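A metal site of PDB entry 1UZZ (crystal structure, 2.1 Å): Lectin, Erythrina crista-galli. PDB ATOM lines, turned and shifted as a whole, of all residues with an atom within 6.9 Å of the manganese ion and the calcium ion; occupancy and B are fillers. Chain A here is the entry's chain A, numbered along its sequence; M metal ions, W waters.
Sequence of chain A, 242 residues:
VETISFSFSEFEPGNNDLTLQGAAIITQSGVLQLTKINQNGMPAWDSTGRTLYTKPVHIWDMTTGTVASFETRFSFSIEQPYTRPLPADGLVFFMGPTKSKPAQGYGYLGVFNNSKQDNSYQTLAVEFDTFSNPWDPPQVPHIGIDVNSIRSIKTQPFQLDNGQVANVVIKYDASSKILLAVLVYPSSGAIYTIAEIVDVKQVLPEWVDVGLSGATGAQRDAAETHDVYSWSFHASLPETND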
ATOM      1  N   ASP A  89      -9.144 -21.157 -18.219  1.00  0.00           N
ATOM      2  CA  ASP A  89     -10.448 -20.834 -17.743  1.00  0.00           C
ATOM      3  C   ASP A  89     -11.494 -21.383 -18.706  1.00  0.00           C
ATOM      4  O   ASP A  89     -12.691 -21.749 -18.413  1.00  0.00           O
ATOM      5  CB  ASP A  89     -10.600 -19.254 -17.559  1.00  0.00           C
ATOM      6  CG  ASP A  89     -10.252 -18.796 -16.233  1.00  0.00           C
ATOM      7  OD1 ASP A  89      -9.092 -18.204 -16.063  1.00  0.00           O
ATOM      8  OD2 ASP A  89     -10.999 -18.761 -15.342  1.00  0.00           O
ATOM      9  N   GLY A  90     -11.073 -21.400 -19.885  1.00  0.00           N
ATOM     10  CA  GLY A  90     -12.057 -21.964 -20.916  1.00  0.00           C
ATOM     11  C   GLY A  90     -12.057 -21.251 -22.254  1.00  0.00           C
ATOM     12  O   GLY A  90     -11.091 -20.404 -22.613  1.00  0.00           O
ATOM     13  N   TYR A 106      -9.219 -14.197 -18.117  1.00  0.00           N
ATOM     14  CA  TYR A 106      -9.496 -15.073 -16.987  1.00  0.00           C
ATOM     15  C   TYR A 106     -10.916 -15.624 -17.111  1.00  0.00           C
ATOM     16  O   TYR A 106     -11.371 -15.937 -18.201  1.00  0.00           O
ATOM     17  CB  TYR A 106      -9.369 -14.305 -15.664  1.00  0.00           C
ATOM     18  CG  TYR A 106      -8.040 -13.631 -15.472  1.00  0.00           C
ATOM     19  CD1 TYR A 106      -7.942 -12.443 -14.749  1.00  0.00           C
ATOM     20  CD2 TYR A 106      -6.866 -14.163 -16.030  1.00  0.00           C
ATOM     21  CE1 TYR A 106      -6.725 -11.801 -14.582  1.00  0.00           C
ATOM     22  CE2 TYR A 106      -5.637 -13.526 -15.875  1.00  0.00           C
ATOM     23  CZ  TYR A 106      -5.581 -12.339 -15.150  1.00  0.00           C
ATOM     24  OH  TYR A 106      -4.383 -11.695 -14.986  1.00  0.00           O
ATOM     25  N   GLY A 107     -11.598 -15.723 -15.974  1.00  0.00           N
ATOM     26  CA  GLY A 107     -12.963 -16.235 -15.974  1.00  0.00           C
ATOM     27  C   GLY A 107     -13.963 -15.493 -16.839  1.00  0.00           C
ATOM     28  O   GLY A 107     -15.074 -15.985 -17.054  1.00  0.00           O
ATOM     29  N   TYR A 108     -13.599 -14.308 -17.337  1.00  0.00           N
ATOM     30  CA  TYR A 108     -14.505 -13.543 -18.201  1.00  0.00           C
ATOM     31  C   TYR A 108     -14.338 -13.980 -19.652  1.00  0.00           C
ATOM     32  O   TYR A 108     -15.056 -13.513 -20.551  1.00  0.00           O
ATOM     33  CB  TYR A 108     -14.264 -12.047 -18.034  1.00  0.00           C
ATOM     34  CG  TYR A 108     -14.494 -11.578 -16.614  1.00  0.00           C
ATOM     35  CD1 TYR A 108     -15.685 -11.869 -15.957  1.00  0.00           C
ATOM     36  CD2 TYR A 108     -13.498 -10.895 -15.918  1.00  0.00           C
ATOM     37  CE1 TYR A 108     -15.871 -11.503 -14.617  1.00  0.00           C
ATOM     38  CE2 TYR A 108     -13.672 -10.533 -14.590  1.00  0.00           C
ATOM     39  CZ  TYR A 108     -14.863 -10.841 -13.943  1.00  0.00           C
ATOM     40  OH  TYR A 108     -15.047 -10.487 -12.622  1.00  0.00           O
ATOM     41  N   LEU A 109     -13.379 -14.875 -19.865  1.00  0.00           N
ATOM     42  CA  LEU A 109     -13.100 -15.469 -21.182  1.00  0.00           C
ATOM     43  C   LEU A 109     -12.876 -14.515 -22.359  1.00  0.00           C
ATOM     44  O   LEU A 109     -13.074 -14.908 -23.508  1.00  0.00           O
ATOM     45  CB  LEU A 109     -14.239 -16.440 -21.540  1.00  0.00           C
ATOM     46  CG  LEU A 109     -14.493 -17.563 -20.526  1.00  0.00           C
ATOM     47  CD1 LEU A 109     -15.736 -18.352 -20.928  1.00  0.00           C
ATOM     48  CD2 LEU A 109     -13.268 -18.470 -20.462  1.00  0.00           C
ATOM     49  N   GLU A 127     -20.309 -21.010 -23.851  1.00  0.00           N
ATOM     50  CA  GLU A 127     -19.011 -21.256 -23.260  1.00  0.00           C
ATOM     51  C   GLU A 127     -18.780 -22.714 -22.947  1.00  0.00           C
ATOM     52  O   GLU A 127     -19.712 -23.497 -22.855  1.00  0.00           O
ATOM     53  CB  GLU A 127     -18.889 -20.467 -21.949  1.00  0.00           C
ATOM     54  CG  GLU A 127     -20.003 -20.826 -20.964  1.00  0.00           C
ATOM     55  CD  GLU A 127     -19.831 -20.229 -19.594  1.00  0.00           C
ATOM     56  OE1 GLU A 127     -19.701 -18.984 -19.481  1.00  0.00           O
ATOM     57  OE2 GLU A 127     -19.834 -20.996 -18.618  1.00  0.00           O
ATOM     58  N   PHE A 128     -17.501 -23.051 -22.771  1.00  0.00           N
ATOM     59  CA  PHE A 128     -17.048 -24.380 -22.417  1.00  0.00           C
ATOM     60  C   PHE A 128     -16.051 -23.998 -21.342  1.00  0.00           C
ATOM     61  O   PHE A 128     -14.870 -23.789 -21.594  1.00  0.00           O
ATOM     62  CB  PHE A 128     -16.402 -25.054 -23.609  1.00  0.00           C
ATOM     63  CG  PHE A 128     -17.379 -25.377 -24.701  1.00  0.00           C
ATOM     64  CD1 PHE A 128     -18.112 -26.566 -24.662  1.00  0.00           C
ATOM     65  CD2 PHE A 128     -17.628 -24.473 -25.725  1.00  0.00           C
ATOM     66  CE1 PHE A 128     -19.066 -26.843 -25.622  1.00  0.00           C
ATOM     67  CE2 PHE A 128     -18.580 -24.745 -26.694  1.00  0.00           C
ATOM     68  CZ  PHE A 128     -19.305 -25.932 -26.639  1.00  0.00           C
ATOM     69  N   ASP A 129     -16.606 -23.871 -20.150  1.00  0.00           N
ATOM     70  CA  ASP A 129     -15.953 -23.423 -18.937  1.00  0.00           C
ATOM     71  C   ASP A 129     -15.191 -24.471 -18.132  1.00  0.00           C
ATOM     72  O   ASP A 129     -15.788 -25.403 -17.603  1.00  0.00           O
ATOM     73  CB  ASP A 129     -17.030 -22.809 -18.061  1.00  0.00           C
ATOM     74  CG  ASP A 129     -16.495 -21.859 -17.077  1.00  0.00           C
ATOM     75  OD1 ASP A 129     -15.318 -22.031 -16.676  1.00  0.00           O
ATOM     76  OD2 ASP A 129     -17.247 -20.943 -16.691  1.00  0.00           O
ATOM     77  N   THR A 130     -13.876 -24.282 -17.999  1.00  0.00           N
ATOM     78  CA  THR A 130     -13.027 -25.229 -17.278  1.00  0.00           C
ATOM     79  C   THR A 130     -12.700 -24.920 -15.810  1.00  0.00           C
ATOM     80  O   THR A 130     -12.166 -25.778 -15.098  1.00  0.00           O
ATOM     81  CB  THR A 130     -11.692 -25.438 -18.025  1.00  0.00           C
ATOM     82  OG1 THR A 130     -11.063 -24.166 -18.232  1.00  0.00           O
ATOM     83  CG2 THR A 130     -11.927 -26.107 -19.373  1.00  0.00           C
ATOM     84  N   PHE A 131     -12.983 -23.708 -15.348  1.00  0.00           N
ATOM     85  CA  PHE A 131     -12.685 -23.324 -13.962  1.00  0.00           C
ATOM     86  C   PHE A 131     -13.985 -22.847 -13.300  1.00  0.00           C
ATOM     87  O   PHE A 131     -14.804 -22.220 -13.928  1.00  0.00           O
ATOM     88  CB  PHE A 131     -11.635 -22.204 -13.930  1.00  0.00           C
ATOM     89  CG  PHE A 131     -11.241 -21.767 -12.534  1.00  0.00           C
ATOM     90  CD1 PHE A 131     -10.156 -22.362 -11.880  1.00  0.00           C
ATOM     91  CD2 PHE A 131     -11.940 -20.766 -11.873  1.00  0.00           C
ATOM     92  CE1 PHE A 131      -9.777 -21.961 -10.595  1.00  0.00           C
ATOM     93  CE2 PHE A 131     -11.570 -20.355 -10.585  1.00  0.00           C
ATOM     94  CZ  PHE A 131     -10.484 -20.953  -9.945  1.00  0.00           C
ATOM     95  N   SER A 132     -14.163 -23.144 -12.019  1.00  0.00           N
ATOM     96  CA  SER A 132     -15.373 -22.740 -11.334  1.00  0.00           C
ATOM     97  C   SER A 132     -15.178 -21.454 -10.524  1.00  0.00           C
ATOM     98  O   SER A 132     -14.599 -21.487  -9.431  1.00  0.00           O
ATOM     99  CB  SER A 132     -15.858 -23.876 -10.411  1.00  0.00           C
ATOM    100  OG  SER A 132     -17.105 -23.564  -9.806  1.00  0.00           O
ATOM    101  N   ASN A 133     -15.649 -20.330 -11.075  1.00  0.00           N
ATOM    102  CA  ASN A 133     -15.573 -19.032 -10.395  1.00  0.00           C
ATOM    103  C   ASN A 133     -16.763 -18.924  -9.433  1.00  0.00           C
ATOM    104  O   ASN A 133     -17.614 -19.812  -9.401  1.00  0.00           O
ATOM    105  CB  ASN A 133     -15.642 -17.867 -11.401  1.00  0.00           C
ATOM    106  CG  ASN A 133     -14.415 -17.788 -12.283  1.00  0.00           C
ATOM    107  OD1 ASN A 133     -14.331 -18.458 -13.296  1.00  0.00           O
ATOM    108  ND2 ASN A 133     -13.443 -16.974 -11.884  1.00  0.00           N
ATOM    109  N   TRP A 135     -19.435 -17.206  -9.582  1.00  0.00           N
ATOM    110  CA  TRP A 135     -20.724 -17.121 -10.273  1.00  0.00           C
ATOM    111  C   TRP A 135     -21.066 -18.393 -11.050  1.00  0.00           C
ATOM    112  O   TRP A 135     -22.100 -18.457 -11.712  1.00  0.00           O
ATOM    113  CB  TRP A 135     -20.717 -15.936 -11.235  1.00  0.00           C
ATOM    114  CG  TRP A 135     -19.694 -16.096 -12.320  1.00  0.00           C
ATOM    115  CD1 TRP A 135     -19.796 -16.863 -13.442  1.00  0.00           C
ATOM    116  CD2 TRP A 135     -18.378 -15.518 -12.351  1.00  0.00           C
ATOM    117  NE1 TRP A 135     -18.627 -16.796 -14.176  1.00  0.00           N
ATOM    118  CE2 TRP A 135     -17.740 -15.984 -13.533  1.00  0.00           C
ATOM    119  CE3 TRP A 135     -17.675 -14.649 -11.499  1.00  0.00           C
ATOM    120  CZ2 TRP A 135     -16.442 -15.607 -13.879  1.00  0.00           C
ATOM    121  CZ3 TRP A 135     -16.378 -14.286 -11.842  1.00  0.00           C
ATOM    122  CH2 TRP A 135     -15.772 -14.763 -13.026  1.00  0.00           C
ATOM    123  N   ASP A 136     -20.210 -19.397 -10.982  1.00  0.00           N
ATOM    124  CA  ASP A 136     -20.405 -20.652 -11.712  1.00  0.00           C
ATOM    125  C   ASP A 136     -20.992 -21.792 -10.913  1.00  0.00           C
ATOM    126  O   ASP A 136     -20.994 -21.783  -9.683  1.00  0.00           O
ATOM    127  CB  ASP A 136     -19.085 -21.184 -12.233  1.00  0.00           C
ATOM    128  CG  ASP A 136     -18.596 -20.466 -13.447  1.00  0.00           C
ATOM    129  OD1 ASP A 136     -19.397 -20.216 -14.360  1.00  0.00           O
ATOM    130  OD2 ASP A 136     -17.394 -20.168 -13.467  1.00  0.00           O
ATOM    131  N   PRO A 137     -21.492 -22.822 -11.623  1.00  0.00           N
ATOM    132  CA  PRO A 137     -22.035 -23.979 -10.909  1.00  0.00           C
ATOM    133  C   PRO A 137     -20.731 -24.637 -10.436  1.00  0.00           C
ATOM    134  O   PRO A 137     -19.672 -24.363 -10.992  1.00  0.00           O
ATOM    135  CB  PRO A 137     -22.735 -24.761 -12.008  1.00  0.00           C
ATOM    136  CG  PRO A 137     -21.966 -24.410 -13.242  1.00  0.00           C
ATOM    137  CD  PRO A 137     -21.738 -22.928 -13.074  1.00  0.00           C
ATOM    138  N   VAL A 140     -17.046 -28.496 -13.212  1.00  0.00           N
ATOM    139  CA  VAL A 140     -16.308 -28.063 -14.389  1.00  0.00           C
ATOM    140  C   VAL A 140     -15.607 -29.301 -14.921  1.00  0.00           C
ATOM    141  O   VAL A 140     -15.195 -30.167 -14.160  1.00  0.00           O
ATOM    142  CB  VAL A 140     -15.251 -26.981 -14.076  1.00  0.00           C
ATOM    143  CG1 VAL A 140     -15.925 -25.653 -13.759  1.00  0.00           C
ATOM    144  CG2 VAL A 140     -14.374 -27.430 -12.908  1.00  0.00           C
ATOM    145  N   HIS A 142     -18.014 -27.360 -17.868  1.00  0.00           N
ATOM    146  CA  HIS A 142     -19.440 -27.301 -18.149  1.00  0.00           C
ATOM    147  C   HIS A 142     -19.742 -26.435 -19.356  1.00  0.00           C
ATOM    148  O   HIS A 142     -18.974 -25.537 -19.719  1.00  0.00           O
ATOM    149  CB  HIS A 142     -20.206 -26.750 -16.932  1.00  0.00           C
ATOM    150  CG  HIS A 142     -19.790 -25.381 -16.511  1.00  0.00           C
ATOM    151  ND1 HIS A 142     -18.882 -25.151 -15.495  1.00  0.00           N
ATOM    152  CD2 HIS A 142     -20.189 -24.156 -16.943  1.00  0.00           C
ATOM    153  CE1 HIS A 142     -18.736 -23.851 -15.319  1.00  0.00           C
ATOM    154  NE2 HIS A 142     -19.515 -23.229 -16.182  1.00  0.00           N
ATOM    155  N   ILE A 143     -20.856 -26.733 -20.005  1.00  0.00           N
ATOM    156  CA  ILE A 143     -21.270 -25.953 -21.151  1.00  0.00           C
ATOM    157  C   ILE A 143     -22.254 -24.954 -20.562  1.00  0.00           C
ATOM    158  O   ILE A 143     -22.904 -25.244 -19.551  1.00  0.00           O
ATOM    159  CB  ILE A 143     -21.987 -26.811 -22.205  1.00  0.00           C
ATOM    160  CG1 ILE A 143     -21.081 -27.971 -22.636  1.00  0.00           C
ATOM    161  CG2 ILE A 143     -22.354 -25.954 -23.398  1.00  0.00           C
ATOM    162  CD1 ILE A 143     -21.714 -28.910 -23.637  1.00  0.00           C
ATOM    163  N   GLY A 144     -22.351 -23.790 -21.176  1.00  0.00           N
ATOM    164  CA  GLY A 144     -23.269 -22.796 -20.672  1.00  0.00           C
ATOM    165  C   GLY A 144     -23.758 -21.820 -21.734  1.00  0.00           C
ATOM    166  O   GLY A 144     -23.024 -21.466 -22.659  1.00  0.00           O
ATOM    167  N   ASP A 146     -24.796 -18.140 -22.368  1.00  0.00           N
ATOM    168  CA  ASP A 146     -24.627 -16.803 -21.786  1.00  0.00           C
ATOM    169  C   ASP A 146     -25.395 -15.721 -22.534  1.00  0.00           C
ATOM    170  O   ASP A 146     -25.211 -15.524 -23.733  1.00  0.00           O
ATOM    171  CB  ASP A 146     -23.137 -16.414 -21.761  1.00  0.00           C
ATOM    172  CG  ASP A 146     -22.275 -17.390 -20.957  1.00  0.00           C
ATOM    173  OD1 ASP A 146     -22.770 -17.922 -19.941  1.00  0.00           O
ATOM    174  OD2 ASP A 146     -21.100 -17.597 -21.319  1.00  0.00           O
ATOM    175  N   ILE A 150     -21.641 -13.401 -17.970  1.00  0.00           N
ATOM    176  CA  ILE A 150     -20.794 -14.565 -17.836  1.00  0.00           C
ATOM    177  C   ILE A 150     -21.508 -15.567 -16.920  1.00  0.00           C
ATOM    178  O   ILE A 150     -21.096 -16.721 -16.804  1.00  0.00           O
ATOM    179  CB  ILE A 150     -19.421 -14.188 -17.217  1.00  0.00           C
ATOM    180  CG1 ILE A 150     -18.444 -15.366 -17.303  1.00  0.00           C
ATOM    181  CG2 ILE A 150     -19.597 -13.750 -15.768  1.00  0.00           C
ATOM    182  CD1 ILE A 150     -18.095 -15.782 -18.732  1.00  0.00           C
ATOM    183  N   ARG A 151     -22.582 -15.103 -16.273  1.00  0.00           N
ATOM    184  CA  ARG A 151     -23.377 -15.959 -15.381  1.00  0.00           C
ATOM    185  C   ARG A 151     -24.434 -16.623 -16.238  1.00  0.00           C
ATOM    186  O   ARG A 151     -25.533 -16.106 -16.399  1.00  0.00           O
ATOM    187  CB  ARG A 151     -24.069 -15.125 -14.292  1.00  0.00           C
ATOM    188  CG  ARG A 151     -23.157 -14.424 -13.289  1.00  0.00           C
ATOM    189  CD  ARG A 151     -24.005 -13.612 -12.314  1.00  0.00           C
ATOM    190  NE  ARG A 151     -23.208 -12.793 -11.385  1.00  0.00           N
ATOM    191  CZ  ARG A 151     -22.747 -13.208 -10.214  1.00  0.00           C
ATOM    192  NH1 ARG A 151     -22.989 -14.436  -9.798  1.00  0.00           N
ATOM    193  NH2 ARG A 151     -22.044 -12.380  -9.449  1.00  0.00           N
ATOM    194  N   SER A 152     -24.088 -17.776 -16.792  1.00  0.00           N
ATOM    195  CA  SER A 152     -24.968 -18.544 -17.672  1.00  0.00           C
ATOM    196  C   SER A 152     -26.416 -18.664 -17.188  1.00  0.00           C
ATOM    197  O   SER A 152     -26.666 -18.815 -15.988  1.00  0.00           O
ATOM    198  CB  SER A 152     -24.394 -19.942 -17.878  1.00  0.00           C
ATOM    199  OG  SER A 152     -22.994 -19.877 -18.070  1.00  0.00           O
ATOM    200  N   THR A 155     -26.585 -24.176 -17.589  1.00  0.00           N
ATOM    201  CA  THR A 155     -25.329 -24.890 -17.696  1.00  0.00           C
ATOM    202  C   THR A 155     -25.499 -26.398 -17.806  1.00  0.00           C
ATOM    203  O   THR A 155     -26.528 -26.945 -17.417  1.00  0.00           O
ATOM    204  CB  THR A 155     -24.429 -24.610 -16.481  1.00  0.00           C
ATOM    205  OG1 THR A 155     -25.162 -24.878 -15.282  1.00  0.00           O
ATOM    206  CG2 THR A 155     -23.968 -23.163 -16.496  1.00  0.00           C
HETATM  207 MN    MN M   1     -19.375 -20.852 -16.447  1.00  0.00          MN
HETATM  208 CA    CA M   2     -15.411 -19.976 -15.082  1.00  0.00          CA
HETATM  209  O   HOH W   1     -19.274 -18.553 -16.831  1.00  0.00           O
HETATM  210  O   HOH W   2     -21.577 -20.885 -16.324  1.00  0.00           O
HETATM  211  O   HOH W   3     -16.628 -17.962 -16.340  1.00  0.00           O
HETATM  212  O   HOH W   4     -12.937 -19.727 -15.969  1.00  0.00           O
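OD2 of Asp 129 binds the manganese ion (2.1 Å).
The manganese ion is bound by OD1 of Asp 136 (2.2 Å).
Water W2 binds the manganese ion, 2.2 Å away.
The side-chain carboxylate (OE2) of Glu 127 is bound to the manganese ion (2.2 Å).
Water W1 is bound to the manganese ion (2.3 Å).
A ring nitrogen (NE2) of His 142 is bound to the manganese ion (2.4 Å).
Along chain A the residues within 4 Å of the calcium ion span positions 129 to 136.
The nearest printed residue that does not touch the calcium ion is Gly 107 (4.5 Å).
Of the 25 residues printed, 4 come within 4 Å of the manganese ion.
Along chain A the residues within 4 Å of the manganese ion span positions 127 to 142.
The side-chain hydroxyl (OG) of Ser 152 sits close to the side-chain carboxylate (OE2) of Glu 127 (3.4 Å).
OD2 of Asp 146 sits close to OE1 of Glu 127 (2.7 Å).
O of Gly 144 is in hydrogen-bond range of N of Glu 127.
The calcium ion is bound by the side-chain carboxylate (OD2) of Asp 136 (2.6 Å), the side-chain amide oxygen (OD1) of Asn 133 (2.6 Å), the backbone carbonyl oxygen (O) of Phe 131 (2.6 Å), the side-chain carboxylate (OD1) of Asp 129 (2.6 Å), the side-chain carboxylate (OD2) of Asp 129 (2.6 Å), water W4 (2.6 Å) and water W3 (2.7 Å).
Water W1 lies within hydrogen-bond range of O of Ile 150, OE1 of Glu 127 and NE1 of Trp 135.
Water W3 lies within hydrogen-bond range of O of Gly 107 (2.6 Å) and NE1 of Trp 135 (3.2 Å).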
